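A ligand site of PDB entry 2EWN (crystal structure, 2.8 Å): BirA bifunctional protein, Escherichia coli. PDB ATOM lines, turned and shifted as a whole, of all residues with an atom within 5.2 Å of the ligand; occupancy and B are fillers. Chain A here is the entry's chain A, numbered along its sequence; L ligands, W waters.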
ATOM      1  N   SER A  89     -15.173   5.428 -24.720  1.00  0.00           N
ATOM      2  CA  SER A  89     -14.477   6.191 -23.686  1.00  0.00           C
ATOM      3  C   SER A  89     -15.215   7.512 -23.486  1.00  0.00           C
ATOM      4  O   SER A  89     -15.532   8.217 -24.458  1.00  0.00           O
ATOM      5  CB  SER A  89     -13.023   6.506 -24.097  1.00  0.00           C
ATOM      6  OG  SER A  89     -12.442   7.524 -23.289  1.00  0.00           O
ATOM      7  N   THR A  90     -15.483   7.862 -22.241  1.00  0.00           N
ATOM      8  CA  THR A  90     -16.158   9.103 -21.958  1.00  0.00           C
ATOM      9  C   THR A  90     -15.299  10.271 -22.426  1.00  0.00           C
ATOM     10  O   THR A  90     -15.824  11.316 -22.821  1.00  0.00           O
ATOM     11  CB  THR A  90     -16.502   9.250 -20.446  1.00  0.00           C
ATOM     12  OG1 THR A  90     -15.391   8.814 -19.655  1.00  0.00           O
ATOM     13  CG2 THR A  90     -17.723   8.419 -20.104  1.00  0.00           C
ATOM     14  N   ASN A  91     -13.979  10.107 -22.387  1.00  0.00           N
ATOM     15  CA  ASN A  91     -13.103  11.168 -22.841  1.00  0.00           C
ATOM     16  C   ASN A  91     -13.226  11.289 -24.359  1.00  0.00           C
ATOM     17  O   ASN A  91     -13.315  12.407 -24.891  1.00  0.00           O
ATOM     18  CB  ASN A  91     -11.652  10.904 -22.421  1.00  0.00           C
ATOM     19  CG  ASN A  91     -11.300  11.518 -21.050  1.00  0.00           C
ATOM     20  OD1 ASN A  91     -12.186  11.900 -20.279  1.00  0.00           O
ATOM     21  ND2 ASN A  91     -10.002  11.602 -20.761  1.00  0.00           N
ATOM     22  N   GLN A 112     -17.331   1.121 -20.494  1.00  0.00           N
ATOM     23  CA  GLN A 112     -16.381   1.634 -21.467  1.00  0.00           C
ATOM     24  C   GLN A 112     -15.704   0.456 -22.131  1.00  0.00           C
ATOM     25  O   GLN A 112     -15.096  -0.387 -21.477  1.00  0.00           O
ATOM     26  CB  GLN A 112     -15.343   2.526 -20.793  1.00  0.00           C
ATOM     27  CG  GLN A 112     -15.896   3.856 -20.324  1.00  0.00           C
ATOM     28  CD  GLN A 112     -14.790   4.772 -19.890  1.00  0.00           C
ATOM     29  OE1 GLN A 112     -14.765   5.955 -20.230  1.00  0.00           O
ATOM     30  NE2 GLN A 112     -13.847   4.230 -19.131  1.00  0.00           N
ATOM     31  N   ALA A 114     -13.389   0.820 -24.440  1.00  0.00           N
ATOM     32  CA  ALA A 114     -12.017   1.188 -24.734  1.00  0.00           C
ATOM     33  C   ALA A 114     -11.556   2.269 -23.762  1.00  0.00           C
ATOM     34  O   ALA A 114     -10.953   3.278 -24.158  1.00  0.00           O
ATOM     35  CB  ALA A 114     -11.894   1.672 -26.186  1.00  0.00           C
ATOM     36  N   GLY A 115     -11.879   2.040 -22.478  1.00  0.00           N
ATOM     37  CA  GLY A 115     -11.503   2.964 -21.427  1.00  0.00           C
ATOM     38  C   GLY A 115      -9.996   3.077 -21.484  1.00  0.00           C
ATOM     39  O   GLY A 115      -9.311   2.090 -21.741  1.00  0.00           O
ATOM     40  N   ARG A 116      -9.457   4.282 -21.259  1.00  0.00           N
ATOM     41  CA  ARG A 116      -8.018   4.444 -21.371  1.00  0.00           C
ATOM     42  C   ARG A 116      -7.305   5.285 -20.313  1.00  0.00           C
ATOM     43  O   ARG A 116      -7.885   6.149 -19.653  1.00  0.00           O
ATOM     44  CB  ARG A 116      -7.671   5.007 -22.754  1.00  0.00           C
ATOM     45  CG  ARG A 116      -8.504   6.220 -23.112  1.00  0.00           C
ATOM     46  CD  ARG A 116      -7.653   7.220 -23.886  1.00  0.00           C
ATOM     47  NE  ARG A 116      -8.326   8.475 -24.236  1.00  0.00           N
ATOM     48  CZ  ARG A 116      -9.134   8.636 -25.290  1.00  0.00           C
ATOM     49  NH1 ARG A 116      -9.375   7.628 -26.108  1.00  0.00           N
ATOM     50  NH2 ARG A 116      -9.674   9.822 -25.541  1.00  0.00           N
ATOM     51  N   GLY A 117      -6.011   5.002 -20.193  1.00  0.00           N
ATOM     52  CA  GLY A 117      -5.172   5.722 -19.260  1.00  0.00           C
ATOM     53  C   GLY A 117      -4.096   6.409 -20.072  1.00  0.00           C
ATOM     54  O   GLY A 117      -4.339   6.745 -21.226  1.00  0.00           O
ATOM     55  N   ARG A 118      -2.927   6.604 -19.488  1.00  0.00           N
ATOM     56  CA  ARG A 118      -1.851   7.236 -20.210  1.00  0.00           C
ATOM     57  C   ARG A 118      -0.949   6.198 -20.874  1.00  0.00           C
ATOM     58  O   ARG A 118      -1.086   4.995 -20.660  1.00  0.00           O
ATOM     59  CB  ARG A 118      -1.080   8.129 -19.269  1.00  0.00           C
ATOM     60  CG  ARG A 118      -1.780   9.441 -18.995  1.00  0.00           C
ATOM     61  CD  ARG A 118      -1.139  10.138 -17.831  1.00  0.00           C
ATOM     62  NE  ARG A 118      -1.483   9.469 -16.582  1.00  0.00           N
ATOM     63  CZ  ARG A 118      -2.579   9.723 -15.876  1.00  0.00           C
ATOM     64  NH1 ARG A 118      -3.451  10.647 -16.295  1.00  0.00           N
ATOM     65  NH2 ARG A 118      -2.813   9.047 -14.758  1.00  0.00           N
ATOM     66  N   ARG A 121      -2.386   2.814 -22.115  1.00  0.00           N
ATOM     67  CA  ARG A 121      -2.894   1.782 -21.232  1.00  0.00           C
ATOM     68  C   ARG A 121      -4.401   1.731 -21.137  1.00  0.00           C
ATOM     69  O   ARG A 121      -5.078   2.688 -21.487  1.00  0.00           O
ATOM     70  CB  ARG A 121      -2.396   1.977 -19.839  1.00  0.00           C
ATOM     71  CG  ARG A 121      -0.896   2.102 -19.745  1.00  0.00           C
ATOM     72  CD  ARG A 121      -0.558   2.207 -18.278  1.00  0.00           C
ATOM     73  NE  ARG A 121       0.832   2.527 -18.071  1.00  0.00           N
ATOM     74  CZ  ARG A 121       1.256   3.716 -17.666  1.00  0.00           C
ATOM     75  NH1 ARG A 121       0.389   4.696 -17.435  1.00  0.00           N
ATOM     76  NH2 ARG A 121       2.539   3.918 -17.484  1.00  0.00           N
ATOM     77  N   LYS A 122      -4.911   0.581 -20.686  1.00  0.00           N
ATOM     78  CA  LYS A 122      -6.347   0.369 -20.570  1.00  0.00           C
ATOM     79  C   LYS A 122      -6.856   0.620 -19.158  1.00  0.00           C
ATOM     80  O   LYS A 122      -6.168   0.322 -18.178  1.00  0.00           O
ATOM     81  CB  LYS A 122      -6.713  -1.069 -21.036  1.00  0.00           C
ATOM     82  CG  LYS A 122      -8.106  -1.197 -21.617  1.00  0.00           C
ATOM     83  CD  LYS A 122      -8.613  -2.632 -21.636  1.00  0.00           C
ATOM     84  CE  LYS A 122     -10.041  -2.697 -22.124  1.00  0.00           C
ATOM     85  NZ  LYS A 122     -10.793  -1.455 -21.798  1.00  0.00           N
ATOM     86  N   TRP A 123      -8.027   1.224 -19.075  1.00  0.00           N
ATOM     87  CA  TRP A 123      -8.688   1.433 -17.808  1.00  0.00           C
ATOM     88  C   TRP A 123      -9.794   0.362 -17.781  1.00  0.00           C
ATOM     89  O   TRP A 123     -10.696   0.393 -18.619  1.00  0.00           O
ATOM     90  CB  TRP A 123      -9.302   2.825 -17.636  1.00  0.00           C
ATOM     91  CG  TRP A 123      -9.791   3.070 -16.234  1.00  0.00           C
ATOM     92  CD1 TRP A 123     -11.104   3.165 -15.794  1.00  0.00           C
ATOM     93  CD2 TRP A 123      -8.970   3.223 -15.073  1.00  0.00           C
ATOM     94  NE1 TRP A 123     -11.130   3.356 -14.416  1.00  0.00           N
ATOM     95  CE2 TRP A 123      -9.843   3.393 -13.951  1.00  0.00           C
ATOM     96  CE3 TRP A 123      -7.584   3.237 -14.860  1.00  0.00           C
ATOM     97  CZ2 TRP A 123      -9.353   3.578 -12.644  1.00  0.00           C
ATOM     98  CZ3 TRP A 123      -7.104   3.414 -13.559  1.00  0.00           C
ATOM     99  CH2 TRP A 123      -7.990   3.579 -12.472  1.00  0.00           C
ATOM    100  N   PHE A 124      -9.680  -0.563 -16.858  1.00  0.00           N
ATOM    101  CA  PHE A 124     -10.665  -1.606 -16.698  1.00  0.00           C
ATOM    102  C   PHE A 124     -11.971  -0.948 -16.294  1.00  0.00           C
ATOM    103  O   PHE A 124     -12.061  -0.331 -15.244  1.00  0.00           O
ATOM    104  CB  PHE A 124     -10.175  -2.604 -15.657  1.00  0.00           C
ATOM    105  CG  PHE A 124     -11.076  -3.761 -15.426  1.00  0.00           C
ATOM    106  CD1 PHE A 124     -11.428  -4.591 -16.482  1.00  0.00           C
ATOM    107  CD2 PHE A 124     -11.570  -4.033 -14.164  1.00  0.00           C
ATOM    108  CE1 PHE A 124     -12.254  -5.679 -16.261  1.00  0.00           C
ATOM    109  CE2 PHE A 124     -12.395  -5.129 -13.937  1.00  0.00           C
ATOM    110  CZ  PHE A 124     -12.737  -5.945 -14.978  1.00  0.00           C
ATOM    111  N   ASN A 130     -18.488   1.020 -11.346  1.00  0.00           N
ATOM    112  CA  ASN A 130     -17.697   2.182 -11.012  1.00  0.00           C
ATOM    113  C   ASN A 130     -18.284   3.416 -11.654  1.00  0.00           C
ATOM    114  O   ASN A 130     -19.236   3.342 -12.437  1.00  0.00           O
ATOM    115  CB  ASN A 130     -16.273   1.976 -11.518  1.00  0.00           C
ATOM    116  CG  ASN A 130     -15.653   0.694 -10.995  1.00  0.00           C
ATOM    117  OD1 ASN A 130     -15.682   0.441  -9.796  1.00  0.00           O
ATOM    118  ND2 ASN A 130     -15.097  -0.115 -11.891  1.00  0.00           N
ATOM    119  N   TYR A 132     -17.665   6.337 -14.272  1.00  0.00           N
ATOM    120  CA  TYR A 132     -16.824   6.726 -15.411  1.00  0.00           C
ATOM    121  C   TYR A 132     -17.363   8.060 -15.904  1.00  0.00           C
ATOM    122  O   TYR A 132     -18.348   8.137 -16.633  1.00  0.00           O
ATOM    123  CB  TYR A 132     -16.907   5.664 -16.525  1.00  0.00           C
ATOM    124  CG  TYR A 132     -16.704   4.256 -16.018  1.00  0.00           C
ATOM    125  CD1 TYR A 132     -15.494   3.858 -15.441  1.00  0.00           C
ATOM    126  CD2 TYR A 132     -17.727   3.330 -16.098  1.00  0.00           C
ATOM    127  CE1 TYR A 132     -15.319   2.563 -14.955  1.00  0.00           C
ATOM    128  CE2 TYR A 132     -17.563   2.022 -15.626  1.00  0.00           C
ATOM    129  CZ  TYR A 132     -16.354   1.645 -15.054  1.00  0.00           C
ATOM    130  OH  TYR A 132     -16.171   0.365 -14.583  1.00  0.00           O
ATOM    131  N   LEU A 133     -16.710   9.125 -15.491  1.00  0.00           N
ATOM    132  CA  LEU A 133     -17.180  10.451 -15.777  1.00  0.00           C
ATOM    133  C   LEU A 133     -16.185  11.375 -16.448  1.00  0.00           C
ATOM    134  O   LEU A 133     -15.010  11.311 -16.170  1.00  0.00           O
ATOM    135  CB  LEU A 133     -17.755  11.016 -14.457  1.00  0.00           C
ATOM    136  CG  LEU A 133     -17.729  12.504 -14.170  1.00  0.00           C
ATOM    137  CD1 LEU A 133     -18.861  13.213 -14.909  1.00  0.00           C
ATOM    138  CD2 LEU A 133     -17.818  12.763 -12.662  1.00  0.00           C
ATOM    139  N   SER A 134     -16.655  12.225 -17.356  1.00  0.00           N
ATOM    140  CA  SER A 134     -15.771  13.191 -18.008  1.00  0.00           C
ATOM    141  C   SER A 134     -16.439  14.562 -18.003  1.00  0.00           C
ATOM    142  O   SER A 134     -17.656  14.661 -18.055  1.00  0.00           O
ATOM    143  CB  SER A 134     -15.468  12.790 -19.451  1.00  0.00           C
ATOM    144  OG  SER A 134     -14.878  11.516 -19.471  1.00  0.00           O
ATOM    145  N   LYS A 172      -1.780  11.941  -6.393  1.00  0.00           N
ATOM    146  CA  LYS A 172      -0.506  11.636  -7.047  1.00  0.00           C
ATOM    147  C   LYS A 172      -0.244  12.741  -8.053  1.00  0.00           C
ATOM    148  O   LYS A 172      -1.120  13.103  -8.842  1.00  0.00           O
ATOM    149  CB  LYS A 172      -0.539  10.286  -7.782  1.00  0.00           C
ATOM    150  CG  LYS A 172       0.581  10.103  -8.849  1.00  0.00           C
ATOM    151  CD  LYS A 172       0.486   8.758  -9.599  1.00  0.00           C
ATOM    152  CE  LYS A 172       0.218   8.956 -11.099  1.00  0.00           C
ATOM    153  NZ  LYS A 172      -0.021   7.674 -11.847  1.00  0.00           N
ATOM    154  N   ASP A 176      -4.490  11.271 -10.619  1.00  0.00           N
ATOM    155  CA  ASP A 176      -4.841  10.016  -9.918  1.00  0.00           C
ATOM    156  C   ASP A 176      -4.918  10.090  -8.393  1.00  0.00           C
ATOM    157  O   ASP A 176      -4.173  10.827  -7.728  1.00  0.00           O
ATOM    158  CB  ASP A 176      -3.849   8.916 -10.288  1.00  0.00           C
ATOM    159  CG  ASP A 176      -3.918   8.484 -11.754  1.00  0.00           C
ATOM    160  OD1 ASP A 176      -4.768   9.022 -12.486  1.00  0.00           O
ATOM    161  OD2 ASP A 176      -3.124   7.617 -12.165  1.00  0.00           O
ATOM    162  N   LYS A 183      -4.345   2.404  -6.245  1.00  0.00           N
ATOM    163  CA  LYS A 183      -5.171   3.302  -7.046  1.00  0.00           C
ATOM    164  C   LYS A 183      -6.663   3.222  -6.805  1.00  0.00           C
ATOM    165  O   LYS A 183      -7.307   2.206  -7.088  1.00  0.00           O
ATOM    166  CB  LYS A 183      -4.912   3.072  -8.547  1.00  0.00           C
ATOM    167  CG  LYS A 183      -4.339   4.289  -9.264  1.00  0.00           C
ATOM    168  CD  LYS A 183      -4.651   4.250 -10.737  1.00  0.00           C
ATOM    169  CE  LYS A 183      -3.379   4.245 -11.567  1.00  0.00           C
ATOM    170  NZ  LYS A 183      -2.436   5.232 -11.000  1.00  0.00           N
ATOM    171  N   GLY A 186      -8.546   6.829 -11.215  1.00  0.00           N
ATOM    172  CA  GLY A 186      -7.613   7.194 -12.244  1.00  0.00           C
ATOM    173  C   GLY A 186      -8.158   8.470 -12.831  1.00  0.00           C
ATOM    174  O   GLY A 186      -9.363   8.580 -13.083  1.00  0.00           O
ATOM    175  N   ILE A 187      -7.298   9.447 -13.075  1.00  0.00           N
ATOM    176  CA  ILE A 187      -7.750  10.699 -13.658  1.00  0.00           C
ATOM    177  C   ILE A 187      -6.900  10.965 -14.876  1.00  0.00           C
ATOM    178  O   ILE A 187      -5.680  10.987 -14.825  1.00  0.00           O
ATOM    179  CB  ILE A 187      -7.623  11.855 -12.672  1.00  0.00           C
ATOM    180  CG1 ILE A 187      -8.582  11.636 -11.506  1.00  0.00           C
ATOM    181  CG2 ILE A 187      -7.928  13.176 -13.351  1.00  0.00           C
ATOM    182  CD1 ILE A 187      -8.627  12.799 -10.531  1.00  0.00           C
ATOM    183  N   LEU A 188      -7.584  11.156 -15.990  1.00  0.00           N
ATOM    184  CA  LEU A 188      -6.927  11.394 -17.255  1.00  0.00           C
ATOM    185  C   LEU A 188      -7.388  12.711 -17.884  1.00  0.00           C
ATOM    186  O   LEU A 188      -8.540  12.828 -18.318  1.00  0.00           O
ATOM    187  CB  LEU A 188      -7.171  10.236 -18.194  1.00  0.00           C
ATOM    188  CG  LEU A 188      -6.709  10.418 -19.643  1.00  0.00           C
ATOM    189  CD1 LEU A 188      -5.182  10.273 -19.751  1.00  0.00           C
ATOM    190  CD2 LEU A 188      -7.391   9.408 -20.563  1.00  0.00           C
ATOM    191  N   GLY A 204     -11.098  13.276 -17.430  1.00  0.00           N
ATOM    192  CA  GLY A 204     -11.726  11.974 -17.268  1.00  0.00           C
ATOM    193  C   GLY A 204     -11.490  11.384 -15.898  1.00  0.00           C
ATOM    194  O   GLY A 204     -10.371  11.411 -15.403  1.00  0.00           O
ATOM    195  N   ALA A 205     -12.531  10.851 -15.280  1.00  0.00           N
ATOM    196  CA  ALA A 205     -12.390  10.253 -13.966  1.00  0.00           C
ATOM    197  C   ALA A 205     -12.924   8.836 -13.946  1.00  0.00           C
ATOM    198  O   ALA A 205     -14.037   8.552 -14.411  1.00  0.00           O
ATOM    199  CB  ALA A 205     -13.115  11.095 -12.916  1.00  0.00           C
ATOM    200  N   GLY A 206     -12.124   7.931 -13.420  1.00  0.00           N
ATOM    201  CA  GLY A 206     -12.499   6.565 -13.277  1.00  0.00           C
ATOM    202  C   GLY A 206     -12.351   6.277 -11.813  1.00  0.00           C
ATOM    203  O   GLY A 206     -11.257   6.006 -11.331  1.00  0.00           O
ATOM    204  N   ASN A 208     -13.130   3.919  -8.618  1.00  0.00           N
ATOM    205  CA  ASN A 208     -13.526   2.567  -8.260  1.00  0.00           C
ATOM    206  C   ASN A 208     -14.496   2.595  -7.073  1.00  0.00           C
ATOM    207  O   ASN A 208     -14.213   3.168  -6.039  1.00  0.00           O
ATOM    208  CB  ASN A 208     -12.305   1.709  -7.941  1.00  0.00           C
ATOM    209  CG  ASN A 208     -11.428   1.488  -9.165  1.00  0.00           C
ATOM    210  OD1 ASN A 208     -11.904   1.499 -10.301  1.00  0.00           O
ATOM    211  ND2 ASN A 208     -10.147   1.268  -8.926  1.00  0.00           N
ATOM    212  N   MET A 211     -16.675  -2.458  -7.520  1.00  0.00           N
ATOM    213  CA  MET A 211     -15.956  -3.505  -8.195  1.00  0.00           C
ATOM    214  C   MET A 211     -15.288  -4.479  -7.184  1.00  0.00           C
ATOM    215  O   MET A 211     -14.469  -4.082  -6.337  1.00  0.00           O
ATOM    216  CB  MET A 211     -14.953  -2.828  -9.157  1.00  0.00           C
ATOM    217  CG  MET A 211     -13.851  -3.760  -9.642  1.00  0.00           C
ATOM    218  SD  MET A 211     -12.504  -2.848 -10.439  1.00  0.00           S
ATOM    219  CE  MET A 211     -13.242  -2.462 -12.022  1.00  0.00           C
ATOM    220  N   VAL A 218      -5.170  -6.724 -16.948  1.00  0.00           N
ATOM    221  CA  VAL A 218      -5.368  -5.311 -17.283  1.00  0.00           C
ATOM    222  C   VAL A 218      -4.875  -4.561 -16.054  1.00  0.00           C
ATOM    223  O   VAL A 218      -4.102  -3.610 -16.162  1.00  0.00           O
ATOM    224  CB  VAL A 218      -6.848  -4.924 -17.516  1.00  0.00           C
ATOM    225  CG1 VAL A 218      -6.924  -3.472 -17.933  1.00  0.00           C
ATOM    226  CG2 VAL A 218      -7.469  -5.810 -18.578  1.00  0.00           C
ATOM    227  N   VAL A 219      -5.317  -5.017 -14.884  1.00  0.00           N
ATOM    228  CA  VAL A 219      -4.922  -4.431 -13.610  1.00  0.00           C
ATOM    229  C   VAL A 219      -3.924  -5.357 -12.912  1.00  0.00           C
ATOM    230  O   VAL A 219      -4.305  -6.326 -12.265  1.00  0.00           O
ATOM    231  CB  VAL A 219      -6.135  -4.238 -12.670  1.00  0.00           C
ATOM    232  CG1 VAL A 219      -5.733  -3.370 -11.489  1.00  0.00           C
ATOM    233  CG2 VAL A 219      -7.293  -3.643 -13.441  1.00  0.00           C
ATOM    234  N   ASN A 220      -2.637  -5.044 -13.059  1.00  0.00           N
ATOM    235  CA  ASN A 220      -1.601  -5.836 -12.428  1.00  0.00           C
ATOM    236  C   ASN A 220      -1.019  -5.109 -11.222  1.00  0.00           C
ATOM    237  O   ASN A 220      -0.272  -5.719 -10.449  1.00  0.00           O
ATOM    238  CB  ASN A 220      -0.490  -6.136 -13.443  1.00  0.00           C
ATOM    239  CG  ASN A 220      -0.518  -5.179 -14.615  1.00  0.00           C
ATOM    240  OD1 ASN A 220      -0.708  -3.978 -14.436  1.00  0.00           O
ATOM    241  ND2 ASN A 220      -0.307  -5.703 -15.820  1.00  0.00           N
ATOM    242  N   GLN A 221      -1.336  -3.822 -11.063  1.00  0.00           N
ATOM    243  CA  GLN A 221      -0.850  -3.061  -9.910  1.00  0.00           C
ATOM    244  C   GLN A 221      -1.919  -3.109  -8.852  1.00  0.00           C
ATOM    245  O   GLN A 221      -2.972  -3.709  -9.076  1.00  0.00           O
ATOM    246  CB  GLN A 221      -0.568  -1.596 -10.245  1.00  0.00           C
ATOM    247  CG  GLN A 221       0.780  -1.347 -10.863  1.00  0.00           C
ATOM    248  CD  GLN A 221       0.646  -0.939 -12.316  1.00  0.00           C
ATOM    249  OE1 GLN A 221       1.614  -0.941 -13.067  1.00  0.00           O
ATOM    250  NE2 GLN A 221      -0.576  -0.566 -12.709  1.00  0.00           N
ATOM    251  N   GLY A 222      -1.659  -2.479  -7.721  1.00  0.00           N
ATOM    252  CA  GLY A 222      -2.638  -2.488  -6.649  1.00  0.00           C
ATOM    253  C   GLY A 222      -3.807  -1.630  -7.050  1.00  0.00           C
ATOM    254  O   GLY A 222      -3.658  -0.719  -7.863  1.00  0.00           O
ATOM    255  N   TRP A 223      -4.967  -1.910  -6.480  1.00  0.00           N
ATOM    256  CA  TRP A 223      -6.181  -1.173  -6.784  1.00  0.00           C
ATOM    257  C   TRP A 223      -7.051  -1.243  -5.554  1.00  0.00           C
ATOM    258  O   TRP A 223      -6.868  -2.130  -4.735  1.00  0.00           O
ATOM    259  CB  TRP A 223      -6.920  -1.781  -7.983  1.00  0.00           C
ATOM    260  CG  TRP A 223      -7.280  -3.218  -7.831  1.00  0.00           C
ATOM    261  CD1 TRP A 223      -6.439  -4.304  -7.965  1.00  0.00           C
ATOM    262  CD2 TRP A 223      -8.556  -3.748  -7.462  1.00  0.00           C
ATOM    263  NE1 TRP A 223      -7.115  -5.473  -7.692  1.00  0.00           N
ATOM    264  CE2 TRP A 223      -8.422  -5.157  -7.383  1.00  0.00           C
ATOM    265  CE3 TRP A 223      -9.799  -3.173  -7.188  1.00  0.00           C
ATOM    266  CZ2 TRP A 223      -9.491  -5.995  -7.042  1.00  0.00           C
ATOM    267  CZ3 TRP A 223     -10.869  -4.010  -6.847  1.00  0.00           C
ATOM    268  CH2 TRP A 223     -10.696  -5.403  -6.771  1.00  0.00           C
ATOM    269  N   GLU A 313       5.933  10.900 -15.338  1.00  0.00           N
ATOM    270  CA  GLU A 313       5.033  10.020 -14.588  1.00  0.00           C
ATOM    271  C   GLU A 313       5.745   9.621 -13.302  1.00  0.00           C
ATOM    272  O   GLU A 313       6.889   9.199 -13.359  1.00  0.00           O
ATOM    273  CB  GLU A 313       4.746   8.761 -15.408  1.00  0.00           C
ATOM    274  CG  GLU A 313       3.410   8.118 -15.110  1.00  0.00           C
ATOM    275  CD  GLU A 313       3.128   6.957 -16.032  1.00  0.00           C
ATOM    276  OE1 GLU A 313       2.096   7.003 -16.744  1.00  0.00           O
ATOM    277  OE2 GLU A 313       3.934   6.012 -16.035  1.00  0.00           O
HETATM  278  P1  LIG L   1      -2.942   5.310 -15.763  1.00  0.00           P
HETATM  279  O1  LIG L   1      -2.450   5.569 -17.175  1.00  0.00           O
HETATM  280  O2  LIG L   1      -1.915   5.762 -14.705  1.00  0.00           O
HETATM  281  O3  LIG L   1      -3.341   3.733 -15.565  1.00  0.00           O
HETATM  282  C1  LIG L   1      -2.442   2.673 -15.710  1.00  0.00           C
HETATM  283  C2  LIG L   1      -2.862   1.447 -15.087  1.00  0.00           C
HETATM  284  O4  LIG L   1      -4.017   1.473 -14.281  1.00  0.00           O
HETATM  285  C3  LIG L   1      -3.188   0.390 -15.993  1.00  0.00           C
HETATM  286  O5  LIG L   1      -2.260  -0.006 -16.981  1.00  0.00           O
HETATM  287  C4  LIG L   1      -3.607  -0.690 -15.056  1.00  0.00           C
HETATM  288  O6  LIG L   1      -2.465  -1.368 -14.614  1.00  0.00           O
HETATM  289  C5  LIG L   1      -4.366   0.084 -13.971  1.00  0.00           C
HETATM  290  N1  LIG L   1      -5.850   0.031 -13.956  1.00  0.00           N
HETATM  291  C6  LIG L   1      -6.719  -0.166 -15.009  1.00  0.00           C
HETATM  292  N2  LIG L   1      -7.978  -0.104 -14.554  1.00  0.00           N
HETATM  293  C7  LIG L   1      -7.938   0.120 -13.195  1.00  0.00           C
HETATM  294  C8  LIG L   1      -8.970   0.294 -12.272  1.00  0.00           C
HETATM  295  N3  LIG L   1     -10.256   0.222 -12.639  1.00  0.00           N
HETATM  296  N4  LIG L   1      -8.577   0.527 -10.910  1.00  0.00           N
HETATM  297  C9  LIG L   1      -7.238   0.607 -10.512  1.00  0.00           C
HETATM  298  N5  LIG L   1      -6.220   0.441 -11.469  1.00  0.00           N
HETATM  299  C10 LIG L   1      -6.610   0.220 -12.802  1.00  0.00           C
HETATM  300  C11 LIG L   1      -4.752   7.151 -15.542  1.00  0.00           C
HETATM  301  O7  LIG L   1      -4.259   5.939 -15.494  1.00  0.00           O
HETATM  302  C12 LIG L   1      -6.233   7.249 -15.299  1.00  0.00           C
HETATM  303  C13 LIG L   1      -7.241   6.391 -16.060  1.00  0.00           C
HETATM  304  C14 LIG L   1      -8.407   7.240 -16.547  1.00  0.00           C
HETATM  305  C15 LIG L   1      -9.766   6.549 -16.421  1.00  0.00           C
HETATM  306  C16 LIG L   1     -10.990   7.415 -16.760  1.00  0.00           C
HETATM  307  S1  LIG L   1     -12.531   6.497 -16.784  1.00  0.00           S
HETATM  308  C17 LIG L   1     -13.384   7.960 -17.326  1.00  0.00           C
HETATM  309  C18 LIG L   1     -12.447   8.486 -18.432  1.00  0.00           C
HETATM  310  N6  LIG L   1     -12.648   7.811 -19.728  1.00  0.00           N
HETATM  311  C19 LIG L   1     -11.488   7.232 -20.143  1.00  0.00           C
HETATM  312  O8  LIG L   1     -11.340   6.598 -21.220  1.00  0.00           O
HETATM  313  N7  LIG L   1     -10.480   7.436 -19.224  1.00  0.00           N
HETATM  314  C20 LIG L   1     -10.963   8.201 -18.101  1.00  0.00           C
HETATM  315  O   HOH W   1       0.194   4.948 -12.995  1.00  0.00           O
HETATM  316  O   HOH W   2      -3.457   0.567 -10.646  1.00  0.00           O
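The backbone carbonyl oxygen of Leu 133 is in hydrogen-bond range of the backbone NH of Ala 205.
N of Gly 204 lies close to OD1 of Asn 91 (3.3 Å).
The side-chain amide nitrogen (ND2) of Asn 91 lies within hydrogen-bond range of the backbone carbonyl oxygen (O) of Leu 188.
The guanidinium group (NH1) of Arg 118 lies within hydrogen-bond range of the backbone carbonyl oxygen (O) of Ile 187 (2.7 Å).
O of Leu 188 lies within hydrogen-bond range of N of Gly 204, at 2.7 Å.
The backbone NH (N) of Trp 123 is in hydrogen-bond range of the backbone carbonyl oxygen (O) of Gly 115 (3.1 Å).
OD2 of Asp 176 lies within salt-bridge range of NZ of Lys 172 (3.1 Å).
The side-chain hydroxyl (OG1) of Thr 90 sits at hydrogen-bond distance from the side-chain hydroxyl (OG) of Ser 134 (2.8 Å).
An oxygen (O1) of the ligand lies within salt-bridge range of the guanidinium group (NH1) of Arg 121 (3.0 Å).
A nitrogen (N6) of the ligand lies within hydrogen-bond range of the side-chain amide oxygen (OE1) of Gln 112, at 2.9 Å.
NZ of Lys 183 lies within salt-bridge range of O2 of the ligand, 3.8 Å away.
A nitrogen (N2) of the ligand sits at hydrogen-bond distance from the backbone NH (N) of Phe 124 (2.9 Å).
A nitrogen (N7) of the ligand sits at hydrogen-bond distance from the backbone carbonyl oxygen of Arg 116, 2.9 Å away.
An oxygen (O1) of the ligand sits at hydrogen-bond distance from the backbone NH (N) of Arg 118 (2.6 Å).
An oxygen (O6) of the ligand lies within hydrogen-bond range of the side-chain amide nitrogen (NE2) of Gln 221, 2.8 Å away.
The backbone carbonyl oxygen of Phe 124 sits at hydrogen-bond distance from a nitrogen (N3) of the ligand (3.2 Å).
NH2 of Arg 118 lies within salt-bridge range of O2 of the ligand.
The side-chain hydroxyl of Ser 89 sits at hydrogen-bond distance from an oxygen (O8) of the ligand.
An oxygen (O6) of the ligand sits close to the backbone carbonyl oxygen (O) of Val 218, at 3.2 Å.
N of Arg 116 is in hydrogen-bond range of O8 of the ligand (3.0 Å).
An oxygen (O6) of the ligand is in hydrogen-bond range of the side-chain amide oxygen of Asn 220 (3.2 Å).
The side-chain amide nitrogen of Asn 208 lies within hydrogen-bond range of a nitrogen (N4) of the ligand, 2.6 Å away.
The backbone NH (N) of Gly 206 lies close to a sulfur (S1) of the ligand (3.7 Å).
The side-chain amino group (NZ) of Lys 172 is in salt-bridge range of an oxygen (O2) of the ligand (3.9 Å).
N6 of the ligand lies within hydrogen-bond range of OG1 of Thr 90 (2.9 Å).
The side-chain carboxylate (OD2) of Asp 176 sits close to an oxygen (O2) of the ligand.
A sulfur (S1) of the ligand sits close to the backbone carbonyl oxygen of Ala 205, 3.5 Å away.
Merely in contact with the ligand: Lys 122 (3.3 Å), Ile 187 (3.3 Å), Trp 123 (3.3 Å), Gly 186 (3.4 Å), Gly 117 (3.4 Å), Trp 223 (3.5 Å), Leu 188 (3.6 Å), Gly 115 (3.6 Å), Gly 204 (3.7 Å), Asn 91 (3.8 Å), Val 219 (3.8 Å) and Leu 133 (3.9 Å).
Hydrophobic or aromatic side chains within 4 Å of the ligand: Trp 123, Phe 124, Leu 188, Val 219 and Trp 223.
The nearest printed residue that does not touch the ligand is Ser 134 (4.02 Å).
Water W1 lies within hydrogen-bond range of an oxygen (O2) of the ligand, the side-chain amino group of Lys 172 and the side-chain amino group of Lys 183.
Water W2 bridges N5 of the ligand (2.9 Å) and O of Gly 222 (3.1 Å).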
